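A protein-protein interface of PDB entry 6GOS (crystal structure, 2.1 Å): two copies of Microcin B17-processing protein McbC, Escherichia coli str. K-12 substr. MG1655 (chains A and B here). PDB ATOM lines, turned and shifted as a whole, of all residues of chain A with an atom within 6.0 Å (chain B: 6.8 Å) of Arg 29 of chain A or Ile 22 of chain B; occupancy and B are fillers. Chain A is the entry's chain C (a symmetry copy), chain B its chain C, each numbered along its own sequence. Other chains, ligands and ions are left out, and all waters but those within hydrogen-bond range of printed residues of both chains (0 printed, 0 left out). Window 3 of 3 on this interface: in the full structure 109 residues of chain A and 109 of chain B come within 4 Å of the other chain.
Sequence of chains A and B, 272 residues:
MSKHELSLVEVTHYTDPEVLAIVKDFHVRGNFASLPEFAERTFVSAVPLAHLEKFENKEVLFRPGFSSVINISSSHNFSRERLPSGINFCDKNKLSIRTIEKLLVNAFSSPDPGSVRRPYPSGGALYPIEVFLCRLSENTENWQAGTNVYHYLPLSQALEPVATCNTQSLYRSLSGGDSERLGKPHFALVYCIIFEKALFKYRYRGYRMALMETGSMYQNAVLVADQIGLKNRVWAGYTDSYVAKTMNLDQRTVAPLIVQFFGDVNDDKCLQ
Arg 29 of chain A touches just these residues of chain B: Ile 22 (3.5 Å) and Tyr 204 (3.6 Å). Printed residues of chain B within 4 Å of Gly 30 of chain A: Tyr 204, Arg 205 and Arg 208. Of chain A, only Arg 29 comes within 4 Å of Ile 22 of chain B. Printed residues of chain A within 4 Å of Val 23 of chain B: Phe 26. Printed residues of chain A within 4 Å of Phe 26 of chain B: Phe 26 (3.4 Å). Arg 203 of chain B touches none of the printed residues of chain A. Printed residues of chain A within 4 Å of Tyr 204 of chain B: Arg 29 (3.6 Å) and Gly 30 (3.7 Å).
OD1 of Asn 31 of chain A is in hydrogen-bond range of NH2 of Arg 208 of chain B, 3.1 Å away. The guanidinium group of Arg 205 of chain B is in hydrogen-bond range of the backbone carbonyl oxygen of Gly 30 of chain A (2.7 Å). NH2 of Arg 208 of chain B sits at hydrogen-bond distance from O of Gly 30 of chain A, at 3.4 Å.
Val 23 of chain B touches Phe 26 of chain A (CA to CE1, 3.999 Å). Phe 26 of chain A touches Phe 26 of chain B (CD2 to CD2, 3.4 Å). His 27 of chain A touches Arg 208 of chain B (NE2 to NH2, 3.6 Å). CG2 of Ile 22 of chain B touches NE of Arg 29 of chain A, 3.5 Å away. Arg 29 of chain A touches Tyr 204 of chain B (CD to CE1, 3.6 Å). CB of Tyr 204 of chain B touches N of Gly 30 of chain A (3.7 Å). NH1 of Arg 205 of chain B touches CA of Asn 31 of chain A, 3.5 Å away.
Phe 26 of chain B touches its own counterpart, Phe 26 of chain A.
Of the 8 printed residues of chain A, 5 touch a printed residue of chain B. Of the 15 printed residues of chain B, 6 touch a printed residue of chain A. Among the printed residues, no Asp or Glu carboxylate lies within 4 Å of a Lys or Arg side-chain nitrogen of the other chain.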
ATOM      1  N   LYS A  24      25.820   7.307 -22.605  1.00  0.00           N
ATOM      2  CA  LYS A  24      26.302   8.631 -22.210  1.00  0.00           C
ATOM      3  C   LYS A  24      26.315   9.621 -23.375  1.00  0.00           C
ATOM      4  O   LYS A  24      25.947  10.789 -23.227  1.00  0.00           O
ATOM      5  CB  LYS A  24      27.706   8.543 -21.629  1.00  0.00           C
ATOM      6  CG  LYS A  24      27.798   7.973 -20.221  1.00  0.00           C
ATOM      7  CD  LYS A  24      29.277   7.715 -19.946  1.00  0.00           C
ATOM      8  CE  LYS A  24      29.582   7.486 -18.501  1.00  0.00           C
ATOM      9  NZ  LYS A  24      31.052   7.712 -18.273  1.00  0.00           N
ATOM     10  N   ASP A  25      26.789   9.164 -24.527  1.00  0.00           N
ATOM     11  CA  ASP A  25      26.864  10.016 -25.717  1.00  0.00           C
ATOM     12  C   ASP A  25      25.491  10.537 -26.070  1.00  0.00           C
ATOM     13  O   ASP A  25      25.366  11.666 -26.514  1.00  0.00           O
ATOM     14  CB  ASP A  25      27.336   9.244 -26.937  1.00  0.00           C
ATOM     15  CG  ASP A  25      28.798   8.969 -26.931  1.00  0.00           C
ATOM     16  OD1 ASP A  25      29.561   9.575 -26.131  1.00  0.00           O
ATOM     17  OD2 ASP A  25      29.180   8.128 -27.778  1.00  0.00           O
ATOM     18  N   PHE A  26      24.487   9.676 -25.936  1.00  0.00           N
ATOM     19  CA  PHE A  26      23.119  10.061 -26.219  1.00  0.00           C
ATOM     20  C   PHE A  26      22.581  10.990 -25.144  1.00  0.00           C
ATOM     21  O   PHE A  26      21.991  12.020 -25.451  1.00  0.00           O
ATOM     22  CB  PHE A  26      22.195   8.851 -26.332  1.00  0.00           C
ATOM     23  CG  PHE A  26      20.756   9.246 -26.508  1.00  0.00           C
ATOM     24  CD1 PHE A  26      20.318   9.768 -27.733  1.00  0.00           C
ATOM     25  CD2 PHE A  26      19.868   9.177 -25.459  1.00  0.00           C
ATOM     26  CE1 PHE A  26      19.006  10.178 -27.901  1.00  0.00           C
ATOM     27  CE2 PHE A  26      18.553   9.570 -25.625  1.00  0.00           C
ATOM     28  CZ  PHE A  26      18.123  10.072 -26.849  1.00  0.00           C
ATOM     29  N   HIS A  27      22.756  10.597 -23.891  1.00  0.00           N
ATOM     30  CA  HIS A  27      22.229  11.351 -22.756  1.00  0.00           C
ATOM     31  C   HIS A  27      22.626  12.817 -22.759  1.00  0.00           C
ATOM     32  O   HIS A  27      21.797  13.714 -22.548  1.00  0.00           O
ATOM     33  CB  HIS A  27      22.712  10.734 -21.451  1.00  0.00           C
ATOM     34  CG  HIS A  27      22.184  11.423 -20.243  1.00  0.00           C
ATOM     35  ND1 HIS A  27      20.974  11.099 -19.674  1.00  0.00           N
ATOM     36  CD2 HIS A  27      22.696  12.432 -19.500  1.00  0.00           C
ATOM     37  CE1 HIS A  27      20.762  11.877 -18.630  1.00  0.00           C
ATOM     38  NE2 HIS A  27      21.796  12.685 -18.492  1.00  0.00           N
ATOM     39  N   VAL A  28      23.901  13.048 -23.013  1.00  0.00           N
ATOM     40  CA  VAL A  28      24.448  14.396 -23.028  1.00  0.00           C
ATOM     41  C   VAL A  28      23.799  15.290 -24.118  1.00  0.00           C
ATOM     42  O   VAL A  28      23.801  16.518 -23.989  1.00  0.00           O
ATOM     43  CB  VAL A  28      25.999  14.340 -23.117  1.00  0.00           C
ATOM     44  CG1 VAL A  28      26.479  14.061 -24.532  1.00  0.00           C
ATOM     45  CG2 VAL A  28      26.611  15.612 -22.587  1.00  0.00           C
ATOM     46  N   ARG A  29      23.234  14.691 -25.170  1.00  0.00           N
ATOM     47  CA  ARG A  29      22.521  15.457 -26.197  1.00  0.00           C
ATOM     48  C   ARG A  29      21.352  16.263 -25.607  1.00  0.00           C
ATOM     49  O   ARG A  29      21.067  17.375 -26.080  1.00  0.00           O
ATOM     50  CB  ARG A  29      22.035  14.585 -27.341  1.00  0.00           C
ATOM     51  CG  ARG A  29      23.149  13.954 -28.150  1.00  0.00           C
ATOM     52  CD  ARG A  29      22.541  13.196 -29.310  1.00  0.00           C
ATOM     53  NE  ARG A  29      23.502  12.407 -30.075  1.00  0.00           N
ATOM     54  CZ  ARG A  29      24.378  12.891 -30.951  1.00  0.00           C
ATOM     55  NH1 ARG A  29      24.509  14.197 -31.168  1.00  0.00           N
ATOM     56  NH2 ARG A  29      25.180  12.050 -31.590  1.00  0.00           N
ATOM     57  N   GLY A  30      20.729  15.728 -24.564  1.00  0.00           N
ATOM     58  CA  GLY A  30      19.677  16.421 -23.852  1.00  0.00           C
ATOM     59  C   GLY A  30      20.034  17.333 -22.678  1.00  0.00           C
ATOM     60  O   GLY A  30      19.125  17.838 -21.999  1.00  0.00           O
ATOM     61  N   ASN A  31      21.319  17.534 -22.419  1.00  0.00           N
ATOM     62  CA  ASN A  31      21.760  18.466 -21.389  1.00  0.00           C
ATOM     63  C   ASN A  31      21.557  19.893 -21.884  1.00  0.00           C
ATOM     64  O   ASN A  31      21.688  20.161 -23.083  1.00  0.00           O
ATOM     65  CB  ASN A  31      23.247  18.256 -21.066  1.00  0.00           C
ATOM     66  CG  ASN A  31      23.504  17.027 -20.192  1.00  0.00           C
ATOM     67  OD1 ASN A  31      22.585  16.311 -19.753  1.00  0.00           O
ATOM     68  ND2 ASN A  31      24.761  16.797 -19.919  1.00  0.00           N
ATOM     69  N   PRO B  17      14.560  16.998 -38.256  1.00  0.00           N
ATOM     70  CA  PRO B  17      14.736  15.609 -38.684  1.00  0.00           C
ATOM     71  C   PRO B  17      16.030  14.934 -38.177  1.00  0.00           C
ATOM     72  O   PRO B  17      16.071  13.722 -38.093  1.00  0.00           O
ATOM     73  CB  PRO B  17      14.770  15.717 -40.215  1.00  0.00           C
ATOM     74  CG  PRO B  17      15.309  17.078 -40.467  1.00  0.00           C
ATOM     75  CD  PRO B  17      14.792  17.948 -39.354  1.00  0.00           C
ATOM     76  N   GLU B  18      17.069  15.707 -37.898  1.00  0.00           N
ATOM     77  CA  GLU B  18      18.295  15.167 -37.318  1.00  0.00           C
ATOM     78  C   GLU B  18      18.016  14.653 -35.885  1.00  0.00           C
ATOM     79  O   GLU B  18      18.397  13.536 -35.505  1.00  0.00           O
ATOM     80  CB  GLU B  18      19.396  16.241 -37.333  1.00  0.00           C
ATOM     81  CG  GLU B  18      20.772  15.768 -36.851  1.00  0.00           C
ATOM     82  CD  GLU B  18      21.611  15.067 -37.919  1.00  0.00           C
ATOM     83  OE1 GLU B  18      21.167  14.939 -39.085  1.00  0.00           O
ATOM     84  OE2 GLU B  18      22.745  14.645 -37.588  1.00  0.00           O
ATOM     85  N   VAL B  19      17.333  15.464 -35.101  1.00  0.00           N
ATOM     86  CA  VAL B  19      16.973  15.070 -33.744  1.00  0.00           C
ATOM     87  C   VAL B  19      16.170  13.782 -33.789  1.00  0.00           C
ATOM     88  O   VAL B  19      16.464  12.856 -33.031  1.00  0.00           O
ATOM     89  CB  VAL B  19      16.140  16.156 -33.025  1.00  0.00           C
ATOM     90  CG1 VAL B  19      15.727  15.689 -31.634  1.00  0.00           C
ATOM     91  CG2 VAL B  19      16.914  17.454 -32.910  1.00  0.00           C
ATOM     92  N   LEU B  20      15.158  13.723 -34.674  1.00  0.00           N
ATOM     93  CA  LEU B  20      14.221  12.605 -34.727  1.00  0.00           C
ATOM     94  C   LEU B  20      14.928  11.321 -35.086  1.00  0.00           C
ATOM     95  O   LEU B  20      14.673  10.309 -34.463  1.00  0.00           O
ATOM     96  CB  LEU B  20      13.099  12.844 -35.726  1.00  0.00           C
ATOM     97  CG  LEU B  20      12.073  11.718 -35.886  1.00  0.00           C
ATOM     98  CD1 LEU B  20      11.273  11.517 -34.616  1.00  0.00           C
ATOM     99  CD2 LEU B  20      11.172  12.035 -37.069  1.00  0.00           C
ATOM    100  N   ALA B  21      15.818  11.377 -36.074  1.00  0.00           N
ATOM    101  CA  ALA B  21      16.597  10.203 -36.488  1.00  0.00           C
ATOM    102  C   ALA B  21      17.521   9.721 -35.393  1.00  0.00           C
ATOM    103  O   ALA B  21      17.618   8.514 -35.178  1.00  0.00           O
ATOM    104  CB  ALA B  21      17.421  10.494 -37.730  1.00  0.00           C
ATOM    105  N   ILE B  22      18.219  10.646 -34.728  1.00  0.00           N
ATOM    106  CA  ILE B  22      19.192  10.271 -33.692  1.00  0.00           C
ATOM    107  C   ILE B  22      18.500   9.645 -32.471  1.00  0.00           C
ATOM    108  O   ILE B  22      19.002   8.658 -31.898  1.00  0.00           O
ATOM    109  CB  ILE B  22      20.098  11.469 -33.328  1.00  0.00           C
ATOM    110  CG1 ILE B  22      21.038  11.737 -34.507  1.00  0.00           C
ATOM    111  CG2 ILE B  22      20.877  11.232 -32.025  1.00  0.00           C
ATOM    112  CD1 ILE B  22      21.965  12.934 -34.353  1.00  0.00           C
ATOM    113  N   VAL B  23      17.355  10.206 -32.079  1.00  0.00           N
ATOM    114  CA  VAL B  23      16.536   9.639 -30.999  1.00  0.00           C
ATOM    115  C   VAL B  23      15.992   8.216 -31.327  1.00  0.00           C
ATOM    116  O   VAL B  23      16.067   7.322 -30.490  1.00  0.00           O
ATOM    117  CB  VAL B  23      15.371  10.577 -30.632  1.00  0.00           C
ATOM    118  CG1 VAL B  23      14.395   9.906 -29.672  1.00  0.00           C
ATOM    119  CG2 VAL B  23      15.895  11.884 -30.044  1.00  0.00           C
ATOM    120  N   LYS B  24      15.419   8.026 -32.518  1.00  0.00           N
ATOM    121  CA  LYS B  24      14.963   6.702 -32.940  1.00  0.00           C
ATOM    122  C   LYS B  24      16.097   5.677 -32.981  1.00  0.00           C
ATOM    123  O   LYS B  24      15.935   4.526 -32.571  1.00  0.00           O
ATOM    124  CB  LYS B  24      14.314   6.768 -34.315  1.00  0.00           C
ATOM    125  CG  LYS B  24      12.920   7.376 -34.354  1.00  0.00           C
ATOM    126  CD  LYS B  24      12.579   7.600 -35.826  1.00  0.00           C
ATOM    127  CE  LYS B  24      11.128   7.864 -36.065  1.00  0.00           C
ATOM    128  NZ  LYS B  24      10.820   7.602 -37.514  1.00  0.00           N
ATOM    129  N   ASP B  25      17.236   6.087 -33.525  1.00  0.00           N
ATOM    130  CA  ASP B  25      18.396   5.197 -33.634  1.00  0.00           C
ATOM    131  C   ASP B  25      18.803   4.705 -32.265  1.00  0.00           C
ATOM    132  O   ASP B  25      19.220   3.568 -32.128  1.00  0.00           O
ATOM    133  CB  ASP B  25      19.612   5.919 -34.189  1.00  0.00           C
ATOM    134  CG  ASP B  25      19.541   6.152 -35.656  1.00  0.00           C
ATOM    135  OD1 ASP B  25      18.686   5.549 -36.360  1.00  0.00           O
ATOM    136  OD2 ASP B  25      20.391   6.956 -36.104  1.00  0.00           O
ATOM    137  N   PHE B  26      18.744   5.598 -31.282  1.00  0.00           N
ATOM    138  CA  PHE B  26      19.086   5.244 -29.919  1.00  0.00           C
ATOM    139  C   PHE B  26      18.013   4.364 -29.300  1.00  0.00           C
ATOM    140  O   PHE B  26      18.319   3.342 -28.695  1.00  0.00           O
ATOM    141  CB  PHE B  26      19.279   6.475 -29.038  1.00  0.00           C
ATOM    142  CG  PHE B  26      19.516   6.116 -27.598  1.00  0.00           C
ATOM    143  CD1 PHE B  26      20.746   5.571 -27.206  1.00  0.00           C
ATOM    144  CD2 PHE B  26      18.515   6.242 -26.662  1.00  0.00           C
ATOM    145  CE1 PHE B  26      20.969   5.194 -25.893  1.00  0.00           C
ATOM    146  CE2 PHE B  26      18.736   5.882 -25.346  1.00  0.00           C
ATOM    147  CZ  PHE B  26      19.965   5.356 -24.962  1.00  0.00           C
ATOM    148  N   HIS B  27      16.764   4.788 -29.425  1.00  0.00           N
ATOM    149  CA  HIS B  27      15.636   4.084 -28.820  1.00  0.00           C
ATOM    150  C   HIS B  27      15.577   2.607 -29.172  1.00  0.00           C
ATOM    151  O   HIS B  27      15.383   1.741 -28.307  1.00  0.00           O
ATOM    152  CB  HIS B  27      14.327   4.726 -29.255  1.00  0.00           C
ATOM    153  CG  HIS B  27      13.128   4.088 -28.648  1.00  0.00           C
ATOM    154  ND1 HIS B  27      12.630   4.463 -27.422  1.00  0.00           N
ATOM    155  CD2 HIS B  27      12.331   3.088 -29.092  1.00  0.00           C
ATOM    156  CE1 HIS B  27      11.576   3.724 -27.135  1.00  0.00           C
ATOM    157  NE2 HIS B  27      11.364   2.891 -28.136  1.00  0.00           N
ATOM    158  N   ARG B 203      13.470  19.355 -28.118  1.00  0.00           N
ATOM    159  CA  ARG B 203      14.490  18.558 -28.770  1.00  0.00           C
ATOM    160  C   ARG B 203      14.860  17.346 -27.900  1.00  0.00           C
ATOM    161  O   ARG B 203      13.969  16.749 -27.270  1.00  0.00           O
ATOM    162  CB  ARG B 203      15.665  19.444 -29.142  1.00  0.00           C
ATOM    163  CG  ARG B 203      15.292  20.618 -30.034  1.00  0.00           C
ATOM    164  CD  ARG B 203      16.451  21.602 -30.153  1.00  0.00           C
ATOM    165  NE  ARG B 203      17.723  21.011 -30.614  1.00  0.00           N
ATOM    166  CZ  ARG B 203      18.016  20.693 -31.875  1.00  0.00           C
ATOM    167  NH1 ARG B 203      17.151  20.897 -32.863  1.00  0.00           N
ATOM    168  NH2 ARG B 203      19.206  20.177 -32.153  1.00  0.00           N
ATOM    169  N   TYR B 204      16.133  16.984 -27.823  1.00  0.00           N
ATOM    170  CA  TYR B 204      16.555  15.746 -27.137  1.00  0.00           C
ATOM    171  C   TYR B 204      16.073  15.611 -25.711  1.00  0.00           C
ATOM    172  O   TYR B 204      15.669  14.521 -25.280  1.00  0.00           O
ATOM    173  CB  TYR B 204      18.062  15.651 -27.105  1.00  0.00           C
ATOM    174  CG  TYR B 204      18.659  15.489 -28.470  1.00  0.00           C
ATOM    175  CD1 TYR B 204      18.676  14.251 -29.080  1.00  0.00           C
ATOM    176  CD2 TYR B 204      19.207  16.575 -29.152  1.00  0.00           C
ATOM    177  CE1 TYR B 204      19.210  14.098 -30.345  1.00  0.00           C
ATOM    178  CE2 TYR B 204      19.739  16.431 -30.428  1.00  0.00           C
ATOM    179  CZ  TYR B 204      19.735  15.196 -31.014  1.00  0.00           C
ATOM    180  OH  TYR B 204      20.259  15.012 -32.257  1.00  0.00           O
ATOM    181  N   ARG B 205      16.115  16.716 -24.974  1.00  0.00           N
ATOM    182  CA  ARG B 205      15.629  16.725 -23.600  1.00  0.00           C
ATOM    183  C   ARG B 205      14.176  16.296 -23.495  1.00  0.00           C
ATOM    184  O   ARG B 205      13.778  15.715 -22.486  1.00  0.00           O
ATOM    185  CB  ARG B 205      15.794  18.079 -22.949  1.00  0.00           C
ATOM    186  CG  ARG B 205      15.896  18.026 -21.419  1.00  0.00           C
ATOM    187  CD  ARG B 205      16.307  19.410 -20.959  1.00  0.00           C
ATOM    188  NE  ARG B 205      16.572  19.630 -19.536  1.00  0.00           N
ATOM    189  CZ  ARG B 205      17.741  19.448 -18.920  1.00  0.00           C
ATOM    190  NH1 ARG B 205      18.792  18.963 -19.554  1.00  0.00           N
ATOM    191  NH2 ARG B 205      17.852  19.752 -17.633  1.00  0.00           N
ATOM    192  N   ARG B 208      13.783  12.467 -22.851  1.00  0.00           N
ATOM    193  CA  ARG B 208      13.992  12.247 -21.430  1.00  0.00           C
ATOM    194  C   ARG B 208      12.710  12.584 -20.645  1.00  0.00           C
ATOM    195  O   ARG B 208      12.249  11.769 -19.821  1.00  0.00           O
ATOM    196  CB  ARG B 208      15.195  13.087 -20.975  1.00  0.00           C
ATOM    197  CG  ARG B 208      15.655  12.797 -19.576  1.00  0.00           C
ATOM    198  CD  ARG B 208      16.345  13.993 -18.967  1.00  0.00           C
ATOM    199  NE  ARG B 208      17.642  14.271 -19.576  1.00  0.00           N
ATOM    200  CZ  ARG B 208      18.497  15.194 -19.122  1.00  0.00           C
ATOM    201  NH1 ARG B 208      18.183  15.962 -18.070  1.00  0.00           N
ATOM    202  NH2 ARG B 208      19.662  15.362 -19.731  1.00  0.00           N
